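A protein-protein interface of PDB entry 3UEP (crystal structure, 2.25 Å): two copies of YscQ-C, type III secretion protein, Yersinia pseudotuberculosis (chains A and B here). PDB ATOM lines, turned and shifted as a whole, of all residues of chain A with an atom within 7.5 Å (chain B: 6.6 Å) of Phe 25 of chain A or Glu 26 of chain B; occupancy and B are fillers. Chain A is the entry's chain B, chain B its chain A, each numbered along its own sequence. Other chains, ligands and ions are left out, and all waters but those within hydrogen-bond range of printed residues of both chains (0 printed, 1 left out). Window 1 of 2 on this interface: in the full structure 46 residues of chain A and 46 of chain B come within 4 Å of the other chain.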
ATOM      1  N   VAL A  23     -11.780  19.975   5.040  1.00  0.00           N
ATOM      2  CA  VAL A  23     -11.997  18.714   5.754  1.00  0.00           C
ATOM      3  C   VAL A  23     -11.718  18.805   7.269  1.00  0.00           C
ATOM      4  O   VAL A  23     -10.599  19.145   7.685  1.00  0.00           O
ATOM      5  CB  VAL A  23     -11.106  17.601   5.201  1.00  0.00           C
ATOM      6  CG1 VAL A  23     -11.364  17.389   3.691  1.00  0.00           C
ATOM      7  CG2 VAL A  23      -9.642  17.927   5.475  1.00  0.00           C
ATOM      8  N   SER A  24     -12.721  18.476   8.087  1.00  0.00           N
ATOM      9  CA  SER A  24     -12.553  18.486   9.546  1.00  0.00           C
ATOM     10  C   SER A  24     -12.296  17.097  10.146  1.00  0.00           C
ATOM     11  O   SER A  24     -12.798  16.090   9.653  1.00  0.00           O
ATOM     12  CB  SER A  24     -13.795  19.077  10.213  1.00  0.00           C
ATOM     13  OG  SER A  24     -14.101  20.359   9.703  1.00  0.00           O
ATOM     14  N   PHE A  25     -11.542  17.053  11.233  1.00  0.00           N
ATOM     15  CA  PHE A  25     -11.418  15.827  12.002  1.00  0.00           C
ATOM     16  C   PHE A  25     -12.025  16.011  13.357  1.00  0.00           C
ATOM     17  O   PHE A  25     -11.438  16.643  14.237  1.00  0.00           O
ATOM     18  CB  PHE A  25      -9.954  15.404  12.124  1.00  0.00           C
ATOM     19  CG  PHE A  25      -9.299  15.216  10.795  1.00  0.00           C
ATOM     20  CD1 PHE A  25      -9.325  13.980  10.159  1.00  0.00           C
ATOM     21  CD2 PHE A  25      -8.732  16.295  10.142  1.00  0.00           C
ATOM     22  CE1 PHE A  25      -8.742  13.816   8.926  1.00  0.00           C
ATOM     23  CE2 PHE A  25      -8.145  16.127   8.908  1.00  0.00           C
ATOM     24  CZ  PHE A  25      -8.154  14.884   8.298  1.00  0.00           C
ATOM     25  N   GLU A  26     -13.212  15.444  13.522  1.00  0.00           N
ATOM     26  CA  GLU A  26     -13.993  15.655  14.729  1.00  0.00           C
ATOM     27  C   GLU A  26     -13.650  14.598  15.778  1.00  0.00           C
ATOM     28  O   GLU A  26     -13.842  13.397  15.557  1.00  0.00           O
ATOM     29  CB  GLU A  26     -15.491  15.632  14.364  1.00  0.00           C
ATOM     30  CG  GLU A  26     -16.426  16.071  15.465  1.00  0.00           C
ATOM     31  CD  GLU A  26     -17.883  15.869  15.091  1.00  0.00           C
ATOM     32  OE1 GLU A  26     -18.402  14.766  15.339  1.00  0.00           O
ATOM     33  OE2 GLU A  26     -18.503  16.796  14.537  1.00  0.00           O
ATOM     34  N   VAL A  27     -13.142  15.036  16.925  1.00  0.00           N
ATOM     35  CA  VAL A  27     -12.747  14.096  17.968  1.00  0.00           C
ATOM     36  C   VAL A  27     -13.796  13.927  19.059  1.00  0.00           C
ATOM     37  O   VAL A  27     -13.621  13.106  19.953  1.00  0.00           O
ATOM     38  CB  VAL A  27     -11.417  14.499  18.639  1.00  0.00           C
ATOM     39  CG1 VAL A  27     -10.230  14.304  17.666  1.00  0.00           C
ATOM     40  CG2 VAL A  27     -11.487  15.915  19.142  1.00  0.00           C
ATOM     41  N   GLY A  28     -14.882  14.695  18.983  1.00  0.00           N
ATOM     42  CA  GLY A  28     -15.918  14.651  20.001  1.00  0.00           C
ATOM     43  C   GLY A  28     -17.132  15.507  19.658  1.00  0.00           C
ATOM     44  O   GLY A  28     -17.043  16.437  18.833  1.00  0.00           O
ATOM     45  N   GLU A  55     -11.730   7.558  18.344  1.00  0.00           N
ATOM     46  CA  GLU A  55     -12.393   7.638  17.052  1.00  0.00           C
ATOM     47  C   GLU A  55     -12.465   9.072  16.531  1.00  0.00           C
ATOM     48  O   GLU A  55     -12.584  10.030  17.292  1.00  0.00           O
ATOM     49  CB  GLU A  55     -13.803   7.056  17.162  1.00  0.00           C
ATOM     50  CG  GLU A  55     -13.844   5.544  17.310  1.00  0.00           C
ATOM     51  CD  GLU A  55     -14.243   4.855  16.020  1.00  0.00           C
ATOM     52  OE1 GLU A  55     -13.868   3.676  15.834  1.00  0.00           O
ATOM     53  OE2 GLU A  55     -14.937   5.495  15.196  1.00  0.00           O
ATOM     54  N   VAL A  56     -12.413   9.201  15.215  1.00  0.00           N
ATOM     55  CA  VAL A  56     -12.365  10.494  14.560  1.00  0.00           C
ATOM     56  C   VAL A  56     -13.343  10.433  13.403  1.00  0.00           C
ATOM     57  O   VAL A  56     -13.317   9.480  12.621  1.00  0.00           O
ATOM     58  CB  VAL A  56     -10.935  10.762  14.036  1.00  0.00           C
ATOM     59  CG1 VAL A  56     -10.924  11.836  12.961  1.00  0.00           C
ATOM     60  CG2 VAL A  56     -10.026  11.128  15.193  1.00  0.00           C
ATOM     61  N   ARG A  57     -14.241  11.403  13.310  1.00  0.00           N
ATOM     62  CA  ARG A  57     -15.090  11.479  12.131  1.00  0.00           C
ATOM     63  C   ARG A  57     -14.432  12.451  11.156  1.00  0.00           C
ATOM     64  O   ARG A  57     -14.113  13.579  11.527  1.00  0.00           O
ATOM     65  CB  ARG A  57     -16.500  11.946  12.493  1.00  0.00           C
ATOM     66  CG  ARG A  57     -17.192  11.082  13.550  1.00  0.00           C
ATOM     67  CD  ARG A  57     -18.456  11.783  14.111  1.00  0.00           C
ATOM     68  NE  ARG A  57     -19.586  11.657  13.195  1.00  0.00           N
ATOM     69  CZ  ARG A  57     -20.233  12.673  12.626  1.00  0.00           C
ATOM     70  NH1 ARG A  57     -19.894  13.930  12.895  1.00  0.00           N
ATOM     71  NH2 ARG A  57     -21.240  12.426  11.791  1.00  0.00           N
ATOM     72  N   LEU A  58     -14.191  11.998   9.929  1.00  0.00           N
ATOM     73  CA  LEU A  58     -13.713  12.870   8.867  1.00  0.00           C
ATOM     74  C   LEU A  58     -14.881  13.553   8.216  1.00  0.00           C
ATOM     75  O   LEU A  58     -15.781  12.892   7.713  1.00  0.00           O
ATOM     76  CB  LEU A  58     -13.022  12.065   7.779  1.00  0.00           C
ATOM     77  CG  LEU A  58     -11.546  11.755   7.938  1.00  0.00           C
ATOM     78  CD1 LEU A  58     -11.346  10.654   8.996  1.00  0.00           C
ATOM     79  CD2 LEU A  58     -10.994  11.362   6.570  1.00  0.00           C
ATOM     80  N   LEU A  59     -14.844  14.876   8.185  1.00  0.00           N
ATOM     81  CA  LEU A  59     -15.932  15.639   7.609  1.00  0.00           C
ATOM     82  C   LEU A  59     -15.394  16.513   6.482  1.00  0.00           C
ATOM     83  O   LEU A  59     -14.289  17.030   6.576  1.00  0.00           O
ATOM     84  CB  LEU A  59     -16.559  16.519   8.686  1.00  0.00           C
ATOM     85  CG  LEU A  59     -16.938  15.869  10.019  1.00  0.00           C
ATOM     86  CD1 LEU A  59     -17.318  16.948  11.019  1.00  0.00           C
ATOM     87  CD2 LEU A  59     -18.085  14.906   9.835  1.00  0.00           C
ATOM     88  N   ALA A  60     -16.172  16.664   5.415  1.00  0.00           N
ATOM     89  CA  ALA A  60     -15.842  17.609   4.356  1.00  0.00           C
ATOM     90  C   ALA A  60     -16.997  18.570   4.201  1.00  0.00           C
ATOM     91  O   ALA A  60     -18.078  18.184   3.755  1.00  0.00           O
ATOM     92  CB  ALA A  60     -15.590  16.890   3.053  1.00  0.00           C
ATOM     93  N   GLY A  62     -18.563  19.897   6.655  1.00  0.00           N
ATOM     94  CA  GLY A  62     -19.509  19.554   7.701  1.00  0.00           C
ATOM     95  C   GLY A  62     -20.197  18.222   7.483  1.00  0.00           C
ATOM     96  O   GLY A  62     -21.033  17.820   8.287  1.00  0.00           O
ATOM     97  N   GLY A  68     -11.874   7.289  11.478  1.00  0.00           N
ATOM     98  CA  GLY A  68     -10.463   7.070  11.612  1.00  0.00           C
ATOM     99  C   GLY A  68     -10.136   6.956  13.085  1.00  0.00           C
ATOM    100  O   GLY A  68     -11.012   7.038  13.943  1.00  0.00           O
ATOM    101  N   LEU A  70      -7.171   8.252  15.966  1.00  0.00           N
ATOM    102  CA  LEU A  70      -5.986   9.052  16.258  1.00  0.00           C
ATOM    103  C   LEU A  70      -4.783   8.155  16.537  1.00  0.00           C
ATOM    104  O   LEU A  70      -4.899   7.123  17.205  1.00  0.00           O
ATOM    105  CB  LEU A  70      -6.219   9.960  17.461  1.00  0.00           C
ATOM    106  CG  LEU A  70      -7.159  11.130  17.229  1.00  0.00           C
ATOM    107  CD1 LEU A  70      -7.366  11.946  18.511  1.00  0.00           C
ATOM    108  CD2 LEU A  70      -6.597  11.984  16.127  1.00  0.00           C
ATOM    109  N   GLY A  78      -1.644  12.140  14.265  1.00  0.00           N
ATOM    110  CA  GLY A  78      -2.209  11.737  12.997  1.00  0.00           C
ATOM    111  C   GLY A  78      -3.450  10.890  13.211  1.00  0.00           C
ATOM    112  O   GLY A  78      -3.861  10.615  14.342  1.00  0.00           O
ATOM    113  N   VAL A  79      -4.014  10.453  12.091  1.00  0.00           N
ATOM    114  CA  VAL A  79      -5.246   9.685  12.020  1.00  0.00           C
ATOM    115  C   VAL A  79      -5.021   8.559  11.026  1.00  0.00           C
ATOM    116  O   VAL A  79      -4.439   8.795   9.961  1.00  0.00           O
ATOM    117  CB  VAL A  79      -6.371  10.554  11.425  1.00  0.00           C
ATOM    118  CG1 VAL A  79      -7.623   9.737  11.223  1.00  0.00           C
ATOM    119  CG2 VAL A  79      -6.641  11.745  12.302  1.00  0.00           C
ATOM    120  N   ILE A  81      -7.139   6.097   8.673  1.00  0.00           N
ATOM    121  CA  ILE A  81      -8.488   5.910   8.158  1.00  0.00           C
ATOM    122  C   ILE A  81      -8.915   4.470   8.386  1.00  0.00           C
ATOM    123  O   ILE A  81      -8.152   3.544   8.113  1.00  0.00           O
ATOM    124  CB  ILE A  81      -8.543   6.166   6.643  1.00  0.00           C
ATOM    125  CG1 ILE A  81      -8.018   7.568   6.310  1.00  0.00           C
ATOM    126  CG2 ILE A  81      -9.958   5.916   6.116  1.00  0.00           C
ATOM    127  CD1 ILE A  81      -8.803   8.673   6.949  1.00  0.00           C
ATOM    128  N   SER B  24     -19.280  20.584  18.979  1.00  0.00           N
ATOM    129  CA  SER B  24     -18.367  19.593  18.417  1.00  0.00           C
ATOM    130  C   SER B  24     -16.922  20.082  18.563  1.00  0.00           C
ATOM    131  O   SER B  24     -16.676  21.290  18.676  1.00  0.00           O
ATOM    132  CB  SER B  24     -18.723  19.288  16.951  1.00  0.00           C
ATOM    133  OG  SER B  24     -18.523  20.421  16.122  1.00  0.00           O
ATOM    134  N   PHE B  25     -15.976  19.144  18.577  1.00  0.00           N
ATOM    135  CA  PHE B  25     -14.569  19.467  18.816  1.00  0.00           C
ATOM    136  C   PHE B  25     -13.753  18.944  17.651  1.00  0.00           C
ATOM    137  O   PHE B  25     -13.807  17.760  17.343  1.00  0.00           O
ATOM    138  CB  PHE B  25     -14.074  18.840  20.139  1.00  0.00           C
ATOM    139  CG  PHE B  25     -14.919  19.223  21.352  1.00  0.00           C
ATOM    140  CD1 PHE B  25     -14.615  20.351  22.101  1.00  0.00           C
ATOM    141  CD2 PHE B  25     -16.031  18.461  21.718  1.00  0.00           C
ATOM    142  CE1 PHE B  25     -15.398  20.717  23.200  1.00  0.00           C
ATOM    143  CE2 PHE B  25     -16.829  18.821  22.821  1.00  0.00           C
ATOM    144  CZ  PHE B  25     -16.508  19.947  23.565  1.00  0.00           C
ATOM    145  N   GLU B  26     -12.993  19.823  17.008  1.00  0.00           N
ATOM    146  CA  GLU B  26     -12.263  19.459  15.811  1.00  0.00           C
ATOM    147  C   GLU B  26     -10.780  19.716  15.966  1.00  0.00           C
ATOM    148  O   GLU B  26     -10.388  20.710  16.566  1.00  0.00           O
ATOM    149  CB  GLU B  26     -12.772  20.276  14.620  1.00  0.00           C
ATOM    150  CG  GLU B  26     -14.101  19.832  14.092  1.00  0.00           C
ATOM    151  CD  GLU B  26     -14.538  20.619  12.860  1.00  0.00           C
ATOM    152  OE1 GLU B  26     -13.904  21.652  12.540  1.00  0.00           O
ATOM    153  OE2 GLU B  26     -15.516  20.194  12.211  1.00  0.00           O
ATOM    154  N   VAL B  27      -9.957  18.842  15.388  1.00  0.00           N
ATOM    155  CA  VAL B  27      -8.511  19.035  15.415  1.00  0.00           C
ATOM    156  C   VAL B  27      -7.919  18.973  14.015  1.00  0.00           C
ATOM    157  O   VAL B  27      -8.457  18.320  13.132  1.00  0.00           O
ATOM    158  CB  VAL B  27      -7.810  17.963  16.263  1.00  0.00           C
ATOM    159  CG1 VAL B  27      -8.218  18.095  17.695  1.00  0.00           C
ATOM    160  CG2 VAL B  27      -8.170  16.579  15.740  1.00  0.00           C
ATOM    161  N   GLY B  28      -6.799  19.651  13.821  1.00  0.00           N
ATOM    162  CA  GLY B  28      -6.024  19.445  12.624  1.00  0.00           C
ATOM    163  C   GLY B  28      -6.435  20.288  11.442  1.00  0.00           C
ATOM    164  O   GLY B  28      -7.395  21.074  11.517  1.00  0.00           O
ATOM    165  N   ARG B  29      -5.682  20.109  10.352  1.00  0.00           N
ATOM    166  CA  ARG B  29      -5.807  20.905   9.136  1.00  0.00           C
ATOM    167  C   ARG B  29      -7.236  20.929   8.655  1.00  0.00           C
ATOM    168  O   ARG B  29      -8.079  20.138   9.091  1.00  0.00           O
ATOM    169  CB  ARG B  29      -5.031  20.249   7.979  1.00  0.00           C
ATOM    170  CG  ARG B  29      -5.637  18.897   7.552  1.00  0.00           C
ATOM    171  CD  ARG B  29      -4.584  17.918   7.090  1.00  0.00           C
ATOM    172  NE  ARG B  29      -3.917  18.421   5.900  1.00  0.00           N
ATOM    173  CZ  ARG B  29      -2.850  17.863   5.342  1.00  0.00           C
ATOM    174  NH1 ARG B  29      -2.312  16.768   5.871  1.00  0.00           N
ATOM    175  NH2 ARG B  29      -2.320  18.407   4.253  1.00  0.00           N
ATOM    176  N   GLN B  30      -7.501  21.822   7.721  1.00  0.00           N
ATOM    177  CA  GLN B  30      -8.844  21.946   7.199  1.00  0.00           C
ATOM    178  C   GLN B  30      -8.828  21.876   5.679  1.00  0.00           C
ATOM    179  O   GLN B  30      -9.867  22.080   5.048  1.00  0.00           O
ATOM    180  CB  GLN B  30      -9.497  23.240   7.704  1.00  0.00           C
ATOM    181  CG  GLN B  30      -9.492  23.401   9.250  1.00  0.00           C
ATOM    182  CD  GLN B  30     -10.207  24.673   9.715  1.00  0.00           C
ATOM    183  OE1 GLN B  30     -11.442  24.735   9.737  1.00  0.00           O
ATOM    184  NE2 GLN B  30      -9.429  25.698  10.075  1.00  0.00           N
ATOM    185  N   LEU B  32      -7.597  19.452   2.312  1.00  0.00           N
ATOM    186  CA  LEU B  32      -7.000  18.419   1.460  1.00  0.00           C
ATOM    187  C   LEU B  32      -7.454  18.661   0.023  1.00  0.00           C
ATOM    188  O   LEU B  32      -8.633  18.938  -0.218  1.00  0.00           O
ATOM    189  CB  LEU B  32      -7.452  17.021   1.896  1.00  0.00           C
ATOM    190  CG  LEU B  32      -7.038  16.550   3.296  1.00  0.00           C
ATOM    191  CD1 LEU B  32      -7.571  15.164   3.586  1.00  0.00           C
ATOM    192  CD2 LEU B  32      -5.547  16.570   3.434  1.00  0.00           C
ATOM    193  N   ILE B  46      -2.988  10.241   7.717  1.00  0.00           N
ATOM    194  CA  ILE B  46      -3.038  11.660   7.454  1.00  0.00           C
ATOM    195  C   ILE B  46      -2.358  12.372   8.591  1.00  0.00           C
ATOM    196  O   ILE B  46      -2.672  12.148   9.765  1.00  0.00           O
ATOM    197  CB  ILE B  46      -4.467  12.201   7.361  1.00  0.00           C
ATOM    198  CG1 ILE B  46      -5.230  11.510   6.240  1.00  0.00           C
ATOM    199  CG2 ILE B  46      -4.453  13.714   7.118  1.00  0.00           C
ATOM    200  CD1 ILE B  46      -6.720  11.970   6.166  1.00  0.00           C
ATOM    201  N   ASP B  47      -1.404  13.216   8.233  1.00  0.00           N
ATOM    202  CA  ASP B  47      -0.800  14.092   9.200  1.00  0.00           C
ATOM    203  C   ASP B  47      -1.760  15.272   9.375  1.00  0.00           C
ATOM    204  O   ASP B  47      -2.176  15.883   8.385  1.00  0.00           O
ATOM    205  CB  ASP B  47       0.542  14.561   8.667  1.00  0.00           C
ATOM    206  CG  ASP B  47       1.240  15.483   9.613  1.00  0.00           C
ATOM    207  OD1 ASP B  47       1.356  15.122  10.798  1.00  0.00           O
ATOM    208  OD2 ASP B  47       1.648  16.573   9.170  1.00  0.00           O
ATOM    209  N   LEU B  48      -2.126  15.573  10.620  1.00  0.00           N
ATOM    210  CA  LEU B  48      -3.091  16.631  10.909  1.00  0.00           C
ATOM    211  C   LEU B  48      -2.443  18.013  11.012  1.00  0.00           C
ATOM    212  O   LEU B  48      -3.122  19.000  11.297  1.00  0.00           O
ATOM    213  CB  LEU B  48      -3.853  16.326  12.204  1.00  0.00           C
ATOM    214  CG  LEU B  48      -4.785  15.110  12.208  1.00  0.00           C
ATOM    215  CD1 LEU B  48      -5.603  15.078  13.476  1.00  0.00           C
ATOM    216  CD2 LEU B  48      -5.712  15.154  11.017  1.00  0.00           C
ATOM    217  N   GLU B  55      -4.141  22.423  18.306  1.00  0.00           N
ATOM    218  CA  GLU B  55      -5.367  23.214  18.249  1.00  0.00           C
ATOM    219  C   GLU B  55      -6.640  22.369  18.183  1.00  0.00           C
ATOM    220  O   GLU B  55      -6.771  21.473  17.355  1.00  0.00           O
ATOM    221  CB  GLU B  55      -5.320  24.188  17.057  1.00  0.00           C
ATOM    222  CG  GLU B  55      -6.361  25.324  17.115  1.00  0.00           C
ATOM    223  CD  GLU B  55      -6.266  26.292  15.934  1.00  0.00           C
ATOM    224  OE1 GLU B  55      -5.336  27.127  15.917  1.00  0.00           O
ATOM    225  OE2 GLU B  55      -7.128  26.221  15.027  1.00  0.00           O
ATOM    226  N   VAL B  56      -7.584  22.672  19.068  1.00  0.00           N
ATOM    227  CA  VAL B  56      -8.931  22.126  18.973  1.00  0.00           C
ATOM    228  C   VAL B  56      -9.848  23.318  18.714  1.00  0.00           C
ATOM    229  O   VAL B  56      -9.735  24.355  19.373  1.00  0.00           O
ATOM    230  CB  VAL B  56      -9.355  21.409  20.266  1.00  0.00           C
ATOM    231  CG1 VAL B  56     -10.814  20.963  20.193  1.00  0.00           C
ATOM    232  CG2 VAL B  56      -8.447  20.216  20.521  1.00  0.00           C
ATOM    233  N   ARG B  57     -10.731  23.204  17.732  1.00  0.00           N
ATOM    234  CA  ARG B  57     -11.724  24.245  17.515  1.00  0.00           C
ATOM    235  C   ARG B  57     -13.050  23.767  18.089  1.00  0.00           C
ATOM    236  O   ARG B  57     -13.464  22.637  17.849  1.00  0.00           O
ATOM    237  CB  ARG B  57     -11.857  24.579  16.023  1.00  0.00           C
ATOM    238  CG  ARG B  57     -10.626  25.273  15.440  1.00  0.00           C
ATOM    239  CD  ARG B  57     -10.608  25.241  13.916  1.00  0.00           C
ATOM    240  NE  ARG B  57     -10.793  23.896  13.378  1.00  0.00           N
ATOM    241  CZ  ARG B  57      -9.833  22.982  13.274  1.00  0.00           C
ATOM    242  NH1 ARG B  57      -8.595  23.249  13.679  1.00  0.00           N
ATOM    243  NH2 ARG B  57     -10.117  21.793  12.771  1.00  0.00           N
ATOM    244  N   LEU B  58     -13.698  24.624  18.875  1.00  0.00           N
ATOM    245  CA  LEU B  58     -15.029  24.315  19.362  1.00  0.00           C
ATOM    246  C   LEU B  58     -16.054  24.929  18.433  1.00  0.00           C
ATOM    247  O   LEU B  58     -16.032  26.128  18.179  1.00  0.00           O
ATOM    248  CB  LEU B  58     -15.260  24.871  20.765  1.00  0.00           C
ATOM    249  CG  LEU B  58     -14.698  24.111  21.964  1.00  0.00           C
ATOM    250  CD1 LEU B  58     -13.166  24.187  21.983  1.00  0.00           C
ATOM    251  CD2 LEU B  58     -15.299  24.705  23.229  1.00  0.00           C
ATOM    252  N   LEU B  59     -16.962  24.106  17.933  1.00  0.00           N
ATOM    253  CA  LEU B  59     -18.038  24.605  17.113  1.00  0.00           C
ATOM    254  C   LEU B  59     -19.343  24.442  17.895  1.00  0.00           C
ATOM    255  O   LEU B  59     -19.538  23.443  18.584  1.00  0.00           O
ATOM    256  CB  LEU B  59     -18.087  23.856  15.779  1.00  0.00           C
ATOM    257  CG  LEU B  59     -16.796  23.834  14.946  1.00  0.00           C
ATOM    258  CD1 LEU B  59     -16.926  22.825  13.827  1.00  0.00           C
ATOM    259  CD2 LEU B  59     -16.475  25.198  14.379  1.00  0.00           C
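The backbone NH (N) of Val 27 of chain A lies within hydrogen-bond range of the backbone carbonyl oxygen (O) of Phe 25 of chain B (2.8 Å).
The backbone NH (N) of Phe 25 of chain B sits at hydrogen-bond distance from the backbone carbonyl oxygen (O) of Gly 28 of chain A, 2.9 Å away.
The side-chain hydroxyl (OG) of Ser 24 of chain A lies close to the side-chain carboxylate (OE2) of Glu 26 of chain B (2.9 Å).
N of Val 27 of chain B sits at hydrogen-bond distance from O of Phe 25 of chain A, at 2.9 Å.
The backbone NH (N) of Val 23 of chain A sits at hydrogen-bond distance from the backbone carbonyl oxygen (O) of Gln 30 of chain B (2.8 Å).
The backbone NH (N) of Ile 46 of chain B sits at hydrogen-bond distance from the backbone carbonyl oxygen (O) of Val 79 of chain A (3.0 Å).
The backbone carbonyl oxygen of Val 23 of chain A lies close to the backbone carbonyl oxygen of Arg 29 of chain B, at 3.1 Å.
Ser 24 of chain A touches Glu 26 of chain B, and with the chains exchanged Glu 26 of chain A touches Ser 24 of chain B.
Phe 25 of chain A touches Glu 26 of chain B, and with the chains exchanged Glu 26 of chain A touches Phe 25 of chain B.
Phe 25 of chain A touches Val 27 of chain B, and with the chains exchanged Val 27 of chain A touches Phe 25 of chain B.
Leu 59 of chain A touches Glu 26 of chain B, but with the chains exchanged Glu 26 of chain A does not touch Leu 59 of chain B (6.3 Å).
Positions printed for both chains: 24, 25, 26, 27, 28, 55, 56, 57, 58 and 59.
The backbone carbonyl oxygen of Leu 59 of chain B sits at hydrogen-bond distance from the backbone NH of Ser 24 of chain B (2.9 Å).
The guanidinium group (NH2) of Arg 57 of chain B lies within salt-bridge range of the side-chain carboxylate (OE1) of Glu 26 of chain B (3.8 Å).
The backbone carbonyl oxygen (O) of Asp 47 of chain B is in hydrogen-bond range of the guanidinium group (NH1) of Arg 29 of chain B (2.7 Å).
The backbone NH of Arg 29 of chain B is in hydrogen-bond range of the backbone carbonyl oxygen of Leu 48 of chain B (2.9 Å).
The backbone carbonyl oxygen of Leu 59 of chain A sits at hydrogen-bond distance from the backbone NH of Ser 24 of chain A, at 2.6 Å.
OE1 of Glu 26 of chain A lies within salt-bridge range of NH1 of Arg 57 of chain A, at 3.0 Å.
Among the printed residues, merely in contact across the chains: Val 23 of chain A with Leu 32 of chain B (3.7 Å), Phe 25 of chain A with Glu 26 of chain B (3.3 Å), Phe 25 of chain A with Arg 29 of chain B (3.98 Å), Phe 25 of chain A with Ile 46 of chain B (3.9 Å), Phe 25 of chain A with Leu 48 of chain B (3.3 Å), Glu 26 of chain A with Ser 24 of chain B (3.5 Å), Glu 26 of chain A with Phe 25 of chain B (3.4 Å), Val 27 of chain A with Val 27 of chain B (3.6 Å), Gly 28 of chain A with Ser 24 of chain B (3.4 Å), Leu 59 of chain A with Glu 26 of chain B (3.9 Å), Gly 78 of chain A with Ile 46 of chain B (3.3 Å), Val 79 of chain A with Leu 48 of chain B (3.7 Å) and Ile 81 of chain A with Ile 46 of chain B (3.98 Å).
Of chain B, only Glu 26, Val 27, Arg 29, Ile 46 and Leu 48 come within 4 Å of Phe 25 of chain A.
Of the printed residues of chain B, Gly 78 of chain A touches Ile 46 (3.3 Å).
Of the printed residues of chain A, Ser 24 of chain B touches Glu 26 (3.5 Å) and Gly 28 (3.4 Å).
Printed residues of chain A within 4 Å of Glu 26 of chain B: Ser 24, Phe 25 and Leu 59.
Asp 47 of chain B touches none of the printed residues of chain A.
The nearest residue of chain B that does not touch Phe 25 of chain A is Phe 25 of chain B (4.1 Å).
Printed residues of chain B that touch a printed residue of chain A: Ser 24, Phe 25, Glu 26, Val 27, Arg 29, Gln 30, Leu 32, Ile 46 and Leu 48.
Hydrophobic or aromatic side chains of chain B within 4 Å of the printed part of chain A: Phe 25, Val 27, Leu 32, Ile 46 and Leu 48.
Along chain B the printed residues that touch a printed residue of chain A span positions 24 to 48.
Of the 18 printed residues of chain A, 10 touch a printed residue of chain B.
Among the printed residues, no Asp or Glu carboxylate lies within 4 Å of a Lys or Arg side-chain nitrogen of the other chain.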
